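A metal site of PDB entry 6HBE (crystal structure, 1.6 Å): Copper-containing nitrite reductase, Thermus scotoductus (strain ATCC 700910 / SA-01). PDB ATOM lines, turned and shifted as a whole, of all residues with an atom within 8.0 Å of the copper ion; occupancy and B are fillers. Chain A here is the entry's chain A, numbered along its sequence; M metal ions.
Of the 27 residues printed, 4 come within 4 Å of the copper ion.
The side-chain amide nitrogen of Gln 130 sits at hydrogen-bond distance from the backbone carbonyl oxygen of Ser 45, 3.2 Å away. NE2 of His 125 sits at hydrogen-bond distance from OE1 of Glu 385, at 2.8 Å. NE2 of His 75 lies within hydrogen-bond range of OD2 of Asp 71, at 2.9 Å. The backbone NH (N) of His 75 sits close to the side-chain amide nitrogen (ND2) of Asn 69 (3.4 Å). The backbone carbonyl oxygen (O) of His 75 lies within hydrogen-bond range of the backbone NH (N) of Val 93, 2.9 Å away. The backbone NH of Gly 76 lies close to the side-chain sulfur of Cys 115 (3.4 Å). The side-chain hydroxyl (OG1) of Thr 126 lies within hydrogen-bond range of the backbone carbonyl oxygen (O) of Cys 115 (3.5 Å).
The copper ion is bound by OE1 of Gln 130 (2.0 Å), ND1 of His 125 (2.0 Å), ND1 of His 75 (2.0 Å) and SG of Cys 115 (2.2 Å). The copper ion has four donor atoms within binding distance.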
ATOM      1  N   ALA A  28     -10.787  -6.805 -10.552  1.00  0.00           N
ATOM      2  CA  ALA A  28     -10.746  -6.694  -9.105  1.00  0.00           C
ATOM      3  C   ALA A  28     -12.077  -6.164  -8.580  1.00  0.00           C
ATOM      4  O   ALA A  28     -12.580  -5.129  -9.093  1.00  0.00           O
ATOM      5  CB  ALA A  28      -9.609  -5.762  -8.686  1.00  0.00           C
ATOM      6  N   ARG A  29     -12.664  -6.879  -7.611  1.00  0.00           N
ATOM      7  CA  ARG A  29     -13.875  -6.411  -6.933  1.00  0.00           C
ATOM      8  C   ARG A  29     -14.083  -6.848  -5.492  1.00  0.00           C
ATOM      9  O   ARG A  29     -13.272  -7.581  -4.959  1.00  0.00           O
ATOM     10  CB  ARG A  29     -15.109  -6.768  -7.729  1.00  0.00           C
ATOM     11  CG  ARG A  29     -15.082  -8.036  -8.521  1.00  0.00           C
ATOM     12  CD  ARG A  29     -16.515  -8.326  -8.873  1.00  0.00           C
ATOM     13  NE  ARG A  29     -16.676  -8.984 -10.139  1.00  0.00           N
ATOM     14  CZ  ARG A  29     -17.756  -8.889 -10.923  1.00  0.00           C
ATOM     15  NH1 ARG A  29     -18.793  -8.109 -10.603  1.00  0.00           N
ATOM     16  NH2 ARG A  29     -17.790  -9.571 -12.049  1.00  0.00           N
ATOM     17  N   PHE A  44     -12.463  -9.746  -0.911  1.00  0.00           N
ATOM     18  CA  PHE A  44     -12.113  -9.150  -2.191  1.00  0.00           C
ATOM     19  C   PHE A  44     -11.786 -10.292  -3.140  1.00  0.00           C
ATOM     20  O   PHE A  44     -11.309 -11.324  -2.685  1.00  0.00           O
ATOM     21  CB  PHE A  44     -10.863  -8.257  -2.099  1.00  0.00           C
ATOM     22  CG  PHE A  44     -11.009  -6.999  -1.259  1.00  0.00           C
ATOM     23  CD1 PHE A  44     -11.910  -5.997  -1.636  1.00  0.00           C
ATOM     24  CD2 PHE A  44     -10.166  -6.766  -0.168  1.00  0.00           C
ATOM     25  CE1 PHE A  44     -12.030  -4.826  -0.896  1.00  0.00           C
ATOM     26  CE2 PHE A  44     -10.278  -5.589   0.576  1.00  0.00           C
ATOM     27  CZ  PHE A  44     -11.222  -4.623   0.231  1.00  0.00           C
ATOM     28  N   SER A  45     -11.999 -10.103  -4.437  1.00  0.00           N
ATOM     29  CA  SER A  45     -11.732 -11.148  -5.444  1.00  0.00           C
ATOM     30  C   SER A  45     -11.182 -10.607  -6.751  1.00  0.00           C
ATOM     31  O   SER A  45     -11.157  -9.393  -6.975  1.00  0.00           O
ATOM     32  CB  SER A  45     -13.007 -11.938  -5.759  1.00  0.00           C
ATOM     33  OG  SER A  45     -13.850 -11.224  -6.660  1.00  0.00           O
ATOM     34  N   PHE A  46     -10.686 -11.523  -7.579  1.00  0.00           N
ATOM     35  CA  PHE A  46     -10.685 -11.340  -9.023  1.00  0.00           C
ATOM     36  C   PHE A  46     -11.870 -12.129  -9.612  1.00  0.00           C
ATOM     37  O   PHE A  46     -12.032 -13.339  -9.345  1.00  0.00           O
ATOM     38  CB  PHE A  46      -9.358 -11.753  -9.669  1.00  0.00           C
ATOM     39  CG  PHE A  46      -8.162 -10.958  -9.167  1.00  0.00           C
ATOM     40  CD1 PHE A  46      -7.931  -9.681  -9.617  1.00  0.00           C
ATOM     41  CD2 PHE A  46      -7.312 -11.488  -8.201  1.00  0.00           C
ATOM     42  CE1 PHE A  46      -6.858  -8.945  -9.152  1.00  0.00           C
ATOM     43  CE2 PHE A  46      -6.221 -10.775  -7.745  1.00  0.00           C
ATOM     44  CZ  PHE A  46      -6.002  -9.486  -8.213  1.00  0.00           C
ATOM     45  N   ASN A  69     -10.056  -2.415 -12.520  1.00  0.00           N
ATOM     46  CA  ASN A  69     -10.542  -2.258 -11.150  1.00  0.00           C
ATOM     47  C   ASN A  69     -12.010  -1.814 -11.169  1.00  0.00           C
ATOM     48  O   ASN A  69     -12.323  -0.662 -11.458  1.00  0.00           O
ATOM     49  CB  ASN A  69      -9.663  -1.275 -10.360  1.00  0.00           C
ATOM     50  CG  ASN A  69     -10.073  -1.158  -8.910  1.00  0.00           C
ATOM     51  OD1 ASN A  69     -11.123  -1.679  -8.491  1.00  0.00           O
ATOM     52  ND2 ASN A  69      -9.252  -0.435  -8.107  1.00  0.00           N
ATOM     53  N   ASP A  71     -13.918  -1.951  -8.460  1.00  0.00           N
ATOM     54  CA  ASP A  71     -14.280  -1.688  -7.063  1.00  0.00           C
ATOM     55  C   ASP A  71     -14.199  -0.178  -6.720  1.00  0.00           C
ATOM     56  O   ASP A  71     -13.829   0.634  -7.573  1.00  0.00           O
ATOM     57  CB  ASP A  71     -13.340  -2.506  -6.147  1.00  0.00           C
ATOM     58  CG  ASP A  71     -13.925  -2.815  -4.778  1.00  0.00           C
ATOM     59  OD1 ASP A  71     -15.105  -2.471  -4.516  1.00  0.00           O
ATOM     60  OD2 ASP A  71     -13.193  -3.388  -3.940  1.00  0.00           O
ATOM     61  N   VAL A  73     -12.251   0.906  -4.002  1.00  0.00           N
ATOM     62  CA  VAL A  73     -10.919   1.155  -3.434  1.00  0.00           C
ATOM     63  C   VAL A  73      -9.843   0.664  -4.416  1.00  0.00           C
ATOM     64  O   VAL A  73     -10.140  -0.086  -5.349  1.00  0.00           O
ATOM     65  CB  VAL A  73     -10.730   0.504  -2.034  1.00  0.00           C
ATOM     66  CG1 VAL A  73     -11.834   0.951  -1.068  1.00  0.00           C
ATOM     67  CG2 VAL A  73     -10.645  -1.022  -2.112  1.00  0.00           C
ATOM     68  N   THR A  74      -8.619   1.127  -4.204  1.00  0.00           N
ATOM     69  CA  THR A  74      -7.447   0.781  -5.016  1.00  0.00           C
ATOM     70  C   THR A  74      -7.090  -0.704  -4.889  1.00  0.00           C
ATOM     71  O   THR A  74      -7.245  -1.293  -3.820  1.00  0.00           O
ATOM     72  CB  THR A  74      -6.229   1.645  -4.601  1.00  0.00           C
ATOM     73  OG1 THR A  74      -6.504   3.028  -4.875  1.00  0.00           O
ATOM     74  CG2 THR A  74      -4.956   1.279  -5.331  1.00  0.00           C
ATOM     75  N   HIS A  75      -6.687  -1.301  -6.003  1.00  0.00           N
ATOM     76  CA  HIS A  75      -6.242  -2.689  -6.087  1.00  0.00           C
ATOM     77  C   HIS A  75      -4.966  -2.731  -6.962  1.00  0.00           C
ATOM     78  O   HIS A  75      -4.345  -1.693  -7.215  1.00  0.00           O
ATOM     79  CB  HIS A  75      -7.365  -3.575  -6.650  1.00  0.00           C
ATOM     80  CG  HIS A  75      -8.519  -3.736  -5.708  1.00  0.00           C
ATOM     81  ND1 HIS A  75      -8.417  -4.444  -4.534  1.00  0.00           N
ATOM     82  CD2 HIS A  75      -9.790  -3.281  -5.753  1.00  0.00           C
ATOM     83  CE1 HIS A  75      -9.580  -4.426  -3.896  1.00  0.00           C
ATOM     84  NE2 HIS A  75     -10.434  -3.739  -4.631  1.00  0.00           N
ATOM     85  N   GLY A  76      -4.539  -3.924  -7.377  1.00  0.00           N
ATOM     86  CA  GLY A  76      -3.362  -4.064  -8.181  1.00  0.00           C
ATOM     87  C   GLY A  76      -3.109  -5.535  -8.447  1.00  0.00           C
ATOM     88  O   GLY A  76      -3.982  -6.365  -8.206  1.00  0.00           O
ATOM     89  N   LEU A  77      -1.936  -5.849  -8.980  1.00  0.00           N
ATOM     90  CA  LEU A  77      -1.570  -7.257  -9.301  1.00  0.00           C
ATOM     91  C   LEU A  77      -0.075  -7.523  -9.228  1.00  0.00           C
ATOM     92  O   LEU A  77       0.752  -6.715  -9.694  1.00  0.00           O
ATOM     93  CB  LEU A  77      -2.073  -7.632 -10.710  1.00  0.00           C
ATOM     94  CG  LEU A  77      -1.829  -9.070 -11.165  1.00  0.00           C
ATOM     95  CD1 LEU A  77      -2.739 -10.050 -10.427  1.00  0.00           C
ATOM     96  CD2 LEU A  77      -2.114  -9.231 -12.648  1.00  0.00           C
ATOM     97  N   VAL A  93      -3.589   0.654  -8.656  1.00  0.00           N
ATOM     98  CA  VAL A  93      -4.623   0.797  -9.683  1.00  0.00           C
ATOM     99  C   VAL A  93      -5.887   1.401  -9.076  1.00  0.00           C
ATOM    100  O   VAL A  93      -6.620   0.749  -8.343  1.00  0.00           O
ATOM    101  CB  VAL A  93      -4.948  -0.532 -10.348  1.00  0.00           C
ATOM    102  CG1 VAL A  93      -5.971  -0.350 -11.478  1.00  0.00           C
ATOM    103  CG2 VAL A  93      -3.661  -1.164 -10.911  1.00  0.00           C
ATOM    104  N   HIS A 114      -1.646 -12.557  -7.041  1.00  0.00           N
ATOM    105  CA  HIS A 114      -2.441 -11.956  -5.963  1.00  0.00           C
ATOM    106  C   HIS A 114      -2.551 -10.458  -6.120  1.00  0.00           C
ATOM    107  O   HIS A 114      -1.832  -9.858  -6.917  1.00  0.00           O
ATOM    108  CB  HIS A 114      -1.818 -12.330  -4.587  1.00  0.00           C
ATOM    109  CG  HIS A 114      -0.385 -11.913  -4.407  1.00  0.00           C
ATOM    110  ND1 HIS A 114      -0.028 -10.659  -3.984  1.00  0.00           N
ATOM    111  CD2 HIS A 114       0.785 -12.585  -4.561  1.00  0.00           C
ATOM    112  CE1 HIS A 114       1.273 -10.545  -3.927  1.00  0.00           C
ATOM    113  NE2 HIS A 114       1.803 -11.705  -4.254  1.00  0.00           N
ATOM    114  N   CYS A 115      -3.430  -9.824  -5.344  1.00  0.00           N
ATOM    115  CA  CYS A 115      -3.542  -8.358  -5.370  1.00  0.00           C
ATOM    116  C   CYS A 115      -2.258  -7.706  -4.809  1.00  0.00           C
ATOM    117  O   CYS A 115      -1.588  -8.254  -3.897  1.00  0.00           O
ATOM    118  CB  CYS A 115      -4.794  -7.899  -4.622  1.00  0.00           C
ATOM    119  SG  CYS A 115      -5.170  -6.151  -4.953  1.00  0.00           S
ATOM    120  N   ALA A 116      -1.875  -6.584  -5.402  1.00  0.00           N
ATOM    121  CA  ALA A 116      -0.725  -5.780  -4.948  1.00  0.00           C
ATOM    122  C   ALA A 116      -1.029  -4.296  -5.160  1.00  0.00           C
ATOM    123  O   ALA A 116      -0.489  -3.678  -6.061  1.00  0.00           O
ATOM    124  CB  ALA A 116       0.552  -6.207  -5.687  1.00  0.00           C
ATOM    125  N   PRO A 117      -1.890  -3.707  -4.280  1.00  0.00           N
ATOM    126  CA  PRO A 117      -2.003  -2.243  -4.330  1.00  0.00           C
ATOM    127  C   PRO A 117      -0.655  -1.551  -4.094  1.00  0.00           C
ATOM    128  O   PRO A 117      -0.393  -0.510  -4.700  1.00  0.00           O
ATOM    129  CB  PRO A 117      -2.976  -1.916  -3.183  1.00  0.00           C
ATOM    130  CG  PRO A 117      -3.489  -3.237  -2.668  1.00  0.00           C
ATOM    131  CD  PRO A 117      -2.499  -4.279  -3.078  1.00  0.00           C
ATOM    132  N   GLY A 118       0.207  -2.164  -3.261  1.00  0.00           N
ATOM    133  CA  GLY A 118       1.453  -1.600  -2.797  1.00  0.00           C
ATOM    134  C   GLY A 118       1.479  -1.602  -1.275  1.00  0.00           C
ATOM    135  O   GLY A 118       0.438  -1.585  -0.623  1.00  0.00           O
ATOM    136  N   GLY A 121      -1.038  -2.851   1.819  1.00  0.00           N
ATOM    137  CA  GLY A 121      -2.171  -3.474   1.168  1.00  0.00           C
ATOM    138  C   GLY A 121      -1.925  -4.791   0.434  1.00  0.00           C
ATOM    139  O   GLY A 121      -2.876  -5.555   0.210  1.00  0.00           O
ATOM    140  N   ILE A 122      -0.682  -5.042   0.048  1.00  0.00           N
ATOM    141  CA  ILE A 122      -0.342  -6.331  -0.567  1.00  0.00           C
ATOM    142  C   ILE A 122      -0.793  -7.480   0.369  1.00  0.00           C
ATOM    143  O   ILE A 122      -1.513  -8.403  -0.026  1.00  0.00           O
ATOM    144  CB  ILE A 122       1.173  -6.467  -0.822  1.00  0.00           C
ATOM    145  CG1 ILE A 122       1.706  -5.337  -1.746  1.00  0.00           C
ATOM    146  CG2 ILE A 122       1.478  -7.829  -1.401  1.00  0.00           C
ATOM    147  CD1 ILE A 122       3.212  -5.335  -1.894  1.00  0.00           C
ATOM    148  N   ALA A 124      -2.639  -7.126   3.235  1.00  0.00           N
ATOM    149  CA  ALA A 124      -3.988  -7.014   3.739  1.00  0.00           C
ATOM    150  C   ALA A 124      -5.065  -7.509   2.740  1.00  0.00           C
ATOM    151  O   ALA A 124      -6.028  -8.199   3.147  1.00  0.00           O
ATOM    152  CB  ALA A 124      -4.278  -5.591   4.203  1.00  0.00           C
ATOM    153  N   HIS A 125      -4.928  -7.152   1.475  1.00  0.00           N
ATOM    154  CA  HIS A 125      -5.859  -7.601   0.429  1.00  0.00           C
ATOM    155  C   HIS A 125      -5.720  -9.083   0.095  1.00  0.00           C
ATOM    156  O   HIS A 125      -6.736  -9.765  -0.128  1.00  0.00           O
ATOM    157  CB  HIS A 125      -5.702  -6.791  -0.864  1.00  0.00           C
ATOM    158  CG  HIS A 125      -6.232  -5.393  -0.775  1.00  0.00           C
ATOM    159  ND1 HIS A 125      -6.849  -4.785  -1.853  1.00  0.00           N
ATOM    160  CD2 HIS A 125      -6.206  -4.487   0.230  1.00  0.00           C
ATOM    161  CE1 HIS A 125      -7.220  -3.566  -1.485  1.00  0.00           C
ATOM    162  NE2 HIS A 125      -6.808  -3.347  -0.240  1.00  0.00           N
ATOM    163  N   THR A 126      -4.484  -9.595   0.048  1.00  0.00           N
ATOM    164  CA  THR A 126      -4.293 -11.011  -0.243  1.00  0.00           C
ATOM    165  C   THR A 126      -4.998 -11.907   0.761  1.00  0.00           C
ATOM    166  O   THR A 126      -5.677 -12.884   0.377  1.00  0.00           O
ATOM    167  CB  THR A 126      -2.805 -11.370  -0.382  1.00  0.00           C
ATOM    168  OG1 THR A 126      -2.240 -10.656  -1.491  1.00  0.00           O
ATOM    169  CG2 THR A 126      -2.630 -12.908  -0.580  1.00  0.00           C
ATOM    170  N   GLN A 130      -7.940 -12.383  -2.558  1.00  0.00           N
ATOM    171  CA  GLN A 130      -7.527 -11.986  -3.891  1.00  0.00           C
ATOM    172  C   GLN A 130      -6.259 -12.732  -4.289  1.00  0.00           C
ATOM    173  O   GLN A 130      -5.165 -12.208  -4.153  1.00  0.00           O
ATOM    174  CB  GLN A 130      -7.306 -10.468  -3.995  1.00  0.00           C
ATOM    175  CG  GLN A 130      -8.536  -9.667  -4.351  1.00  0.00           C
ATOM    176  CD  GLN A 130      -8.327  -8.139  -4.440  1.00  0.00           C
ATOM    177  OE1 GLN A 130      -7.668  -7.431  -3.598  1.00  0.00           O
ATOM    178  NE2 GLN A 130      -8.941  -7.594  -5.494  1.00  0.00           N
ATOM    179  N   TYR A 314     -12.558  -7.678   7.992  1.00  0.00           N
ATOM    180  CA  TYR A 314     -12.401  -6.234   8.126  1.00  0.00           C
ATOM    181  C   TYR A 314     -13.529  -5.507   8.874  1.00  0.00           C
ATOM    182  O   TYR A 314     -13.293  -4.405   9.382  1.00  0.00           O
ATOM    183  CB  TYR A 314     -12.282  -5.578   6.769  1.00  0.00           C
ATOM    184  CG  TYR A 314     -11.326  -6.265   5.791  1.00  0.00           C
ATOM    185  CD1 TYR A 314      -9.960  -6.325   6.025  1.00  0.00           C
ATOM    186  CD2 TYR A 314     -11.819  -6.794   4.597  1.00  0.00           C
ATOM    187  CE1 TYR A 314      -9.099  -6.925   5.105  1.00  0.00           C
ATOM    188  CE2 TYR A 314     -10.966  -7.399   3.673  1.00  0.00           C
ATOM    189  CZ  TYR A 314      -9.627  -7.442   3.914  1.00  0.00           C
ATOM    190  OH  TYR A 314      -8.810  -8.055   2.970  1.00  0.00           O
ATOM    191  N   GLU A 385      -4.916   2.613   0.282  1.00  0.00           N
ATOM    192  CA  GLU A 385      -4.757   1.154   0.443  1.00  0.00           C
ATOM    193  C   GLU A 385      -3.292   0.717   0.568  1.00  0.00           C
ATOM    194  O   GLU A 385      -3.055  -0.445   0.923  1.00  0.00           O
ATOM    195  CB  GLU A 385      -5.442   0.392  -0.706  1.00  0.00           C
ATOM    196  CG  GLU A 385      -6.951   0.580  -0.753  1.00  0.00           C
ATOM    197  CD  GLU A 385      -7.678   0.130   0.511  1.00  0.00           C
ATOM    198  OE1 GLU A 385      -7.367  -0.974   1.066  1.00  0.00           O
ATOM    199  OE2 GLU A 385      -8.612   0.861   0.921  1.00  0.00           O
ATOM    200  N   TYR A 433     -14.204   0.220   4.165  1.00  0.00           N
ATOM    201  CA  TYR A 433     -14.729  -1.123   4.518  1.00  0.00           C
ATOM    202  C   TYR A 433     -14.407  -1.610   5.954  1.00  0.00           C
ATOM    203  O   TYR A 433     -14.976  -2.593   6.404  1.00  0.00           O
ATOM    204  CB  TYR A 433     -14.268  -2.170   3.477  1.00  0.00           C
ATOM    205  CG  TYR A 433     -12.768  -2.204   3.309  1.00  0.00           C
ATOM    206  CD1 TYR A 433     -12.110  -1.352   2.412  1.00  0.00           C
ATOM    207  CD2 TYR A 433     -11.995  -3.069   4.075  1.00  0.00           C
ATOM    208  CE1 TYR A 433     -10.723  -1.367   2.297  1.00  0.00           C
ATOM    209  CE2 TYR A 433     -10.611  -3.101   3.962  1.00  0.00           C
ATOM    210  CZ  TYR A 433      -9.982  -2.241   3.088  1.00  0.00           C
ATOM    211  OH  TYR A 433      -8.618  -2.264   2.977  1.00  0.00           O
HETATM  212 CU    CU M   1      -6.890  -5.554  -3.745  1.00  0.00          CU
